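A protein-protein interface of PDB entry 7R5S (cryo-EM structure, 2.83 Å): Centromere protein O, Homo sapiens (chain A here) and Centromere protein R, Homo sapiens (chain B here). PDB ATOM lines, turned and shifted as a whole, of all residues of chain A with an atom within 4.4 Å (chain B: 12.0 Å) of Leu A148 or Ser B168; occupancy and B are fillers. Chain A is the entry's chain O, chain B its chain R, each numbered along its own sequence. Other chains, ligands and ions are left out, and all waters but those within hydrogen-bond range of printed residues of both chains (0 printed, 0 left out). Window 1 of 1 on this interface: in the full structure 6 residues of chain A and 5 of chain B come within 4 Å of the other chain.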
ATOM      1  N   VAL A 143      12.008 -12.773 -10.833  1.00  0.00           N
ATOM      2  CA  VAL A 143      11.926 -11.837 -11.947  1.00  0.00           C
ATOM      3  C   VAL A 143      13.341 -11.404 -12.301  1.00  0.00           C
ATOM      4  O   VAL A 143      14.146 -11.111 -11.410  1.00  0.00           O
ATOM      5  CB  VAL A 143      11.048 -10.618 -11.607  1.00  0.00           C
ATOM      6  CG1 VAL A 143      10.796  -9.784 -12.849  1.00  0.00           C
ATOM      7  CG2 VAL A 143       9.732 -11.063 -10.987  1.00  0.00           C
ATOM      8  N   ILE A 144      13.643 -11.364 -13.601  1.00  0.00           N
ATOM      9  CA  ILE A 144      15.007 -11.101 -14.048  1.00  0.00           C
ATOM     10  C   ILE A 144      15.328  -9.614 -14.168  1.00  0.00           C
ATOM     11  O   ILE A 144      16.505  -9.238 -14.071  1.00  0.00           O
ATOM     12  CB  ILE A 144      15.276 -11.800 -15.394  1.00  0.00           C
ATOM     13  CG1 ILE A 144      14.688 -13.210 -15.390  1.00  0.00           C
ATOM     14  CG2 ILE A 144      16.769 -11.874 -15.678  1.00  0.00           C
ATOM     15  CD1 ILE A 144      15.291 -14.123 -14.344  1.00  0.00           C
ATOM     16  N   GLN A 145      14.326  -8.761 -14.372  1.00  0.00           N
ATOM     17  CA  GLN A 145      14.583  -7.335 -14.524  1.00  0.00           C
ATOM     18  C   GLN A 145      15.218  -6.766 -13.259  1.00  0.00           C
ATOM     19  O   GLN A 145      14.953  -7.219 -12.144  1.00  0.00           O
ATOM     20  CB  GLN A 145      13.288  -6.589 -14.853  1.00  0.00           C
ATOM     21  CG  GLN A 145      12.241  -6.611 -13.750  1.00  0.00           C
ATOM     22  CD  GLN A 145      12.328  -5.405 -12.835  1.00  0.00           C
ATOM     23  OE1 GLN A 145      12.911  -4.382 -13.192  1.00  0.00           O
ATOM     24  NE2 GLN A 145      11.748  -5.522 -11.647  1.00  0.00           N
ATOM     25  N   LYS A 146      16.075  -5.769 -13.445  1.00  0.00           N
ATOM     26  CA  LYS A 146      16.804  -5.177 -12.329  1.00  0.00           C
ATOM     27  C   LYS A 146      15.942  -4.126 -11.639  1.00  0.00           C
ATOM     28  O   LYS A 146      15.374  -3.261 -12.312  1.00  0.00           O
ATOM     29  CB  LYS A 146      18.109  -4.550 -12.817  1.00  0.00           C
ATOM     30  CG  LYS A 146      19.160  -4.349 -11.736  1.00  0.00           C
ATOM     31  CD  LYS A 146      19.093  -2.952 -11.139  1.00  0.00           C
ATOM     32  CE  LYS A 146      20.179  -2.746 -10.096  1.00  0.00           C
ATOM     33  NZ  LYS A 146      20.108  -1.394  -9.477  1.00  0.00           N
ATOM     34  N   PRO A 147      15.820  -4.163 -10.302  1.00  0.00           N
ATOM     35  CA  PRO A 147      16.440  -5.164  -9.426  1.00  0.00           C
ATOM     36  C   PRO A 147      15.604  -6.435  -9.303  1.00  0.00           C
ATOM     37  O   PRO A 147      14.391  -6.390  -9.504  1.00  0.00           O
ATOM     38  CB  PRO A 147      16.523  -4.437  -8.086  1.00  0.00           C
ATOM     39  CG  PRO A 147      15.333  -3.542  -8.092  1.00  0.00           C
ATOM     40  CD  PRO A 147      15.112  -3.126  -9.529  1.00  0.00           C
ATOM     41  N   LEU A 148      16.255  -7.551  -8.981  1.00  0.00           N
ATOM     42  CA  LEU A 148      15.554  -8.824  -8.882  1.00  0.00           C
ATOM     43  C   LEU A 148      14.525  -8.789  -7.760  1.00  0.00           C
ATOM     44  O   LEU A 148      14.804  -8.327  -6.651  1.00  0.00           O
ATOM     45  CB  LEU A 148      16.551  -9.959  -8.644  1.00  0.00           C
ATOM     46  CG  LEU A 148      17.745 -10.046  -9.595  1.00  0.00           C
ATOM     47  CD1 LEU A 148      18.645 -11.211  -9.218  1.00  0.00           C
ATOM     48  CD2 LEU A 148      17.279 -10.172 -11.033  1.00  0.00           C
ATOM     49  N   ARG A 149      13.328  -9.281  -8.057  1.00  0.00           N
ATOM     50  CA  ARG A 149      12.231  -9.356  -7.103  1.00  0.00           C
ATOM     51  C   ARG A 149      11.725 -10.793  -7.016  1.00  0.00           C
ATOM     52  O   ARG A 149      12.219 -11.694  -7.696  1.00  0.00           O
ATOM     53  CB  ARG A 149      11.096  -8.405  -7.495  1.00  0.00           C
ATOM     54  CG  ARG A 149      11.549  -7.020  -7.917  1.00  0.00           C
ATOM     55  CD  ARG A 149      10.406  -6.023  -7.830  1.00  0.00           C
ATOM     56  NE  ARG A 149       9.111  -6.656  -8.069  1.00  0.00           N
ATOM     57  CZ  ARG A 149       8.510  -6.708  -9.254  1.00  0.00           C
ATOM     58  NH1 ARG A 149       9.087  -6.162 -10.316  1.00  0.00           N
ATOM     59  NH2 ARG A 149       7.334  -7.305  -9.377  1.00  0.00           N
ATOM     60  N   LEU A 169      20.208 -12.109  -2.548  1.00  0.00           N
ATOM     61  CA  LEU A 169      19.471 -12.142  -3.809  1.00  0.00           C
ATOM     62  C   LEU A 169      20.180 -11.339  -4.892  1.00  0.00           C
ATOM     63  O   LEU A 169      20.209 -11.751  -6.058  1.00  0.00           O
ATOM     64  CB  LEU A 169      18.047 -11.627  -3.608  1.00  0.00           C
ATOM     65  CG  LEU A 169      17.123 -11.670  -4.824  1.00  0.00           C
ATOM     66  CD1 LEU A 169      16.965 -13.095  -5.322  1.00  0.00           C
ATOM     67  CD2 LEU A 169      15.771 -11.065  -4.486  1.00  0.00           C
ATOM     68  N   GLN A 170      20.760 -10.196  -4.532  1.00  0.00           N
ATOM     69  CA  GLN A 170      21.393  -9.323  -5.512  1.00  0.00           C
ATOM     70  C   GLN A 170      22.822  -9.732  -5.846  1.00  0.00           C
ATOM     71  O   GLN A 170      23.395  -9.184  -6.794  1.00  0.00           O
ATOM     72  CB  GLN A 170      21.380  -7.876  -5.012  1.00  0.00           C
ATOM     73  CG  GLN A 170      20.036  -7.417  -4.472  1.00  0.00           C
ATOM     74  CD  GLN A 170      18.949  -7.408  -5.529  1.00  0.00           C
ATOM     75  OE1 GLN A 170      19.223  -7.259  -6.719  1.00  0.00           O
ATOM     76  NE2 GLN A 170      17.704  -7.570  -5.096  1.00  0.00           N
ATOM     77  N   THR A 171      23.403 -10.679  -5.110  1.00  0.00           N
ATOM     78  CA  THR A 171      24.769 -11.127  -5.352  1.00  0.00           C
ATOM     79  C   THR A 171      24.852 -12.621  -5.078  1.00  0.00           C
ATOM     80  O   THR A 171      24.432 -13.077  -4.010  1.00  0.00           O
ATOM     81  CB  THR A 171      25.776 -10.381  -4.467  1.00  0.00           C
ATOM     82  OG1 THR A 171      25.333 -10.406  -3.104  1.00  0.00           O
ATOM     83  CG2 THR A 171      25.952  -8.937  -4.923  1.00  0.00           C
ATOM     84  N   ASN A 172      25.401 -13.371  -6.036  1.00  0.00           N
ATOM     85  CA  ASN A 172      25.594 -14.817  -5.915  1.00  0.00           C
ATOM     86  C   ASN A 172      24.257 -15.524  -5.665  1.00  0.00           C
ATOM     87  O   ASN A 172      23.996 -16.087  -4.600  1.00  0.00           O
ATOM     88  CB  ASN A 172      26.616 -15.142  -4.819  1.00  0.00           C
ATOM     89  CG  ASN A 172      27.394 -16.409  -5.106  1.00  0.00           C
ATOM     90  OD1 ASN A 172      27.357 -16.934  -6.218  1.00  0.00           O
ATOM     91  ND2 ASN A 172      28.110 -16.904  -4.103  1.00  0.00           N
ATOM     92  N   ASP B 167      27.447  -8.006 -10.603  1.00  0.00           N
ATOM     93  CA  ASP B 167      26.643  -8.689  -9.597  1.00  0.00           C
ATOM     94  C   ASP B 167      25.888  -9.883 -10.179  1.00  0.00           C
ATOM     95  O   ASP B 167      26.407 -10.604 -11.031  1.00  0.00           O
ATOM     96  CB  ASP B 167      25.668  -7.702  -8.936  1.00  0.00           C
ATOM     97  CG  ASP B 167      24.765  -6.990  -9.938  1.00  0.00           C
ATOM     98  OD1 ASP B 167      24.328  -5.859  -9.636  1.00  0.00           O
ATOM     99  OD2 ASP B 167      24.489  -7.546 -11.022  1.00  0.00           O
ATOM    100  N   SER B 168      24.657 -10.085  -9.710  1.00  0.00           N
ATOM    101  CA  SER B 168      23.838 -11.206 -10.152  1.00  0.00           C
ATOM    102  C   SER B 168      23.046 -10.890 -11.414  1.00  0.00           C
ATOM    103  O   SER B 168      22.835 -11.777 -12.247  1.00  0.00           O
ATOM    104  CB  SER B 168      22.882 -11.628  -9.034  1.00  0.00           C
ATOM    105  OG  SER B 168      21.898 -10.635  -8.807  1.00  0.00           O
ATOM    106  N   TYR B 169      22.607  -9.639 -11.573  1.00  0.00           N
ATOM    107  CA  TYR B 169      21.782  -9.283 -12.724  1.00  0.00           C
ATOM    108  C   TYR B 169      22.558  -9.435 -14.027  1.00  0.00           C
ATOM    109  O   TYR B 169      22.062 -10.028 -14.991  1.00  0.00           O
ATOM    110  CB  TYR B 169      21.259  -7.855 -12.572  1.00  0.00           C
ATOM    111  CG  TYR B 169      20.574  -7.324 -13.810  1.00  0.00           C
ATOM    112  CD1 TYR B 169      21.213  -6.421 -14.648  1.00  0.00           C
ATOM    113  CD2 TYR B 169      19.288  -7.729 -14.142  1.00  0.00           C
ATOM    114  CE1 TYR B 169      20.591  -5.934 -15.782  1.00  0.00           C
ATOM    115  CE2 TYR B 169      18.658  -7.247 -15.273  1.00  0.00           C
ATOM    116  CZ  TYR B 169      19.314  -6.351 -16.089  1.00  0.00           C
ATOM    117  OH  TYR B 169      18.689  -5.869 -17.216  1.00  0.00           O
ATOM    118  N   GLU B 170      23.781  -8.902 -14.075  1.00  0.00           N
ATOM    119  CA  GLU B 170      24.575  -8.999 -15.295  1.00  0.00           C
ATOM    120  C   GLU B 170      25.007 -10.435 -15.562  1.00  0.00           C
ATOM    121  O   GLU B 170      25.027 -10.879 -16.716  1.00  0.00           O
ATOM    122  CB  GLU B 170      25.787  -8.069 -15.211  1.00  0.00           C
ATOM    123  CG  GLU B 170      26.588  -8.186 -13.923  1.00  0.00           C
ATOM    124  CD  GLU B 170      27.734  -9.173 -14.034  1.00  0.00           C
ATOM    125  OE1 GLU B 170      28.008  -9.642 -15.158  1.00  0.00           O
ATOM    126  OE2 GLU B 170      28.360  -9.478 -12.998  1.00  0.00           O
ATOM    127  N   PHE B 171      25.348 -11.181 -14.507  1.00  0.00           N
ATOM    128  CA  PHE B 171      25.725 -12.580 -14.680  1.00  0.00           C
ATOM    129  C   PHE B 171      24.557 -13.402 -15.209  1.00  0.00           C
ATOM    130  O   PHE B 171      24.752 -14.344 -15.988  1.00  0.00           O
ATOM    131  CB  PHE B 171      26.235 -13.153 -13.357  1.00  0.00           C
ATOM    132  CG  PHE B 171      26.146 -14.652 -13.267  1.00  0.00           C
ATOM    133  CD1 PHE B 171      27.070 -15.453 -13.916  1.00  0.00           C
ATOM    134  CD2 PHE B 171      25.142 -15.258 -12.528  1.00  0.00           C
ATOM    135  CE1 PHE B 171      26.992 -16.830 -13.835  1.00  0.00           C
ATOM    136  CE2 PHE B 171      25.060 -16.635 -12.445  1.00  0.00           C
ATOM    137  CZ  PHE B 171      25.987 -17.422 -13.098  1.00  0.00           C
ATOM    138  N   LEU B 172      23.335 -13.061 -14.798  1.00  0.00           N
ATOM    139  CA  LEU B 172      22.164 -13.784 -15.280  1.00  0.00           C
ATOM    140  C   LEU B 172      21.821 -13.381 -16.709  1.00  0.00           C
ATOM    141  O   LEU B 172      21.439 -14.225 -17.528  1.00  0.00           O
ATOM    142  CB  LEU B 172      20.979 -13.535 -14.345  1.00  0.00           C
ATOM    143  CG  LEU B 172      19.904 -14.621 -14.304  1.00  0.00           C
ATOM    144  CD1 LEU B 172      20.525 -15.970 -13.978  1.00  0.00           C
ATOM    145  CD2 LEU B 172      18.830 -14.265 -13.292  1.00  0.00           C
ATOM    146  N   LYS B 173      21.950 -12.090 -17.026  1.00  0.00           N
ATOM    147  CA  LYS B 173      21.646 -11.614 -18.370  1.00  0.00           C
ATOM    148  C   LYS B 173      22.667 -12.079 -19.398  1.00  0.00           C
ATOM    149  O   LYS B 173      22.314 -12.237 -20.572  1.00  0.00           O
ATOM    150  CB  LYS B 173      21.556 -10.088 -18.380  1.00  0.00           C
ATOM    151  CG  LYS B 173      20.136  -9.554 -18.317  1.00  0.00           C
ATOM    152  CD  LYS B 173      19.338  -9.979 -19.538  1.00  0.00           C
ATOM    153  CE  LYS B 173      17.968  -9.322 -19.561  1.00  0.00           C
ATOM    154  NZ  LYS B 173      17.156  -9.686 -18.367  1.00  0.00           N
ATOM    155  N   ALA B 174      23.918 -12.301 -18.993  1.00  0.00           N
ATOM    156  CA  ALA B 174      24.938 -12.780 -19.919  1.00  0.00           C
ATOM    157  C   ALA B 174      24.737 -14.233 -20.328  1.00  0.00           C
ATOM    158  O   ALA B 174      25.545 -14.752 -21.106  1.00  0.00           O
ATOM    159  CB  ALA B 174      26.327 -12.605 -19.304  1.00  0.00           C
ATOM    160  N   ILE B 175      23.699 -14.896 -19.832  1.00  0.00           N
ATOM    161  CA  ILE B 175      23.430 -16.293 -20.153  1.00  0.00           C
ATOM    162  C   ILE B 175      22.262 -16.430 -21.121  1.00  0.00           C
ATOM    163  O   ILE B 175      22.326 -17.204 -22.077  1.00  0.00           O
ATOM    164  CB  ILE B 175      23.180 -17.098 -18.858  1.00  0.00           C
ATOM    165  CG1 ILE B 175      24.417 -17.063 -17.960  1.00  0.00           C
ATOM    166  CG2 ILE B 175      22.790 -18.524 -19.191  1.00  0.00           C
ATOM    167  CD1 ILE B 175      24.184 -17.630 -16.578  1.00  0.00           C
ATOM    168  N   LEU B 176      21.182 -15.681 -20.886  1.00  0.00           N
ATOM    169  CA  LEU B 176      20.000 -15.786 -21.735  1.00  0.00           C
ATOM    170  C   LEU B 176      20.267 -15.337 -23.166  1.00  0.00           C
ATOM    171  O   LEU B 176      19.500 -15.691 -24.067  1.00  0.00           O
ATOM    172  CB  LEU B 176      18.852 -14.967 -21.141  1.00  0.00           C
ATOM    173  CG  LEU B 176      18.341 -15.408 -19.768  1.00  0.00           C
ATOM    174  CD1 LEU B 176      18.361 -14.245 -18.788  1.00  0.00           C
ATOM    175  CD2 LEU B 176      16.943 -15.995 -19.879  1.00  0.00           C
ATOM    176  N   ASN B 177      21.329 -14.571 -23.394  1.00  0.00           N
ATOM    177  CA  ASN B 177      21.675 -14.124 -24.737  1.00  0.00           C
ATOM    178  C   ASN B 177      22.254 -15.270 -25.559  1.00  0.00           C
ATOM    179  O   ASN B 177      22.567 -16.334 -25.025  1.00  0.00           O
ATOM    180  CB  ASN B 177      22.670 -12.963 -24.676  1.00  0.00           C
ATOM    181  CG  ASN B 177      22.274 -11.911 -23.659  1.00  0.00           C
ATOM    182  OD1 ASN B 177      21.105 -11.790 -23.297  1.00  0.00           O
ATOM    183  ND2 ASN B 177      23.252 -11.144 -23.192  1.00  0.00           N
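Among the printed residues, merely in contact across the chains: Ile A144 with Tyr B169 (3.2 Å), Ile A144 with Leu B172 (3.7 Å), Ile A144 with Lys B173 (3.5 Å), Lys A146 with Tyr B169 (3.5 Å), Leu A148 with Ser B168 (3.3 Å), Gln A170 with Asp B167 (3.5 Å) and Thr A171 with Ser B168 (3.99 Å).
OD2 of Asp B167 sits at hydrogen-bond distance from N of Tyr B169 (2.9 Å). The side-chain carboxylate (OE2) of Glu B170 sits at hydrogen-bond distance from the backbone NH (N) of Asp B167. The backbone carbonyl oxygen (O) of Lys B173 is in hydrogen-bond range of the side-chain amide nitrogen (ND2) of Asn B177, at 3.0 Å. The backbone carbonyl oxygen (O) of Leu A148 lies within hydrogen-bond range of the side-chain amide nitrogen (NE2) of Gln A170 (3.4 Å).
Of the 11 printed residues of chain B, 5 touch a printed residue of chain A. Printed residues of chain B that touch a printed residue of chain A: Asp B167, Ser B168, Tyr B169, Leu B172 and Lys B173. Of the 11 printed residues of chain A, 6 touch a printed residue of chain B. Printed residues of chain A that touch a printed residue of chain B: Ile A144, Lys A146, Leu A148, Leu A169, Gln A170 and Thr A171. Among the printed residues, 9 pairs touch across the chains. Among the printed residues, no Asp or Glu carboxylate lies within 4 Å of a Lys or Arg side-chain nitrogen of the other chain.
Printed residues of chain B within 4 Å of Lys A146: Tyr B169 (3.5 Å). No residue of chain B comes within 4 Å of Pro A147. Of the printed residues of chain B, Leu A148 touches Ser B168 (3.3 Å). No residue of chain B comes within 4 Å of Arg A149. Of chain B, only Ser B168 comes within 4 Å of Leu A169. Asn A172 touches none of the printed residues of chain B. Printed residues of chain A within 4 Å of Asp B167: Gln A170. Printed residues of chain A within 4 Å of Ser B168: Leu A148, Leu A169, Gln A170 and Thr A171. Of the printed residues of chain A, Lys B173 touches Ile A144.
O of Leu A169 lies within hydrogen-bond range of OG of Ser B168, at 3.4 Å. The backbone carbonyl oxygen of Gln A170 lies within hydrogen-bond range of the side-chain hydroxyl of Ser B168, at 2.9 Å.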
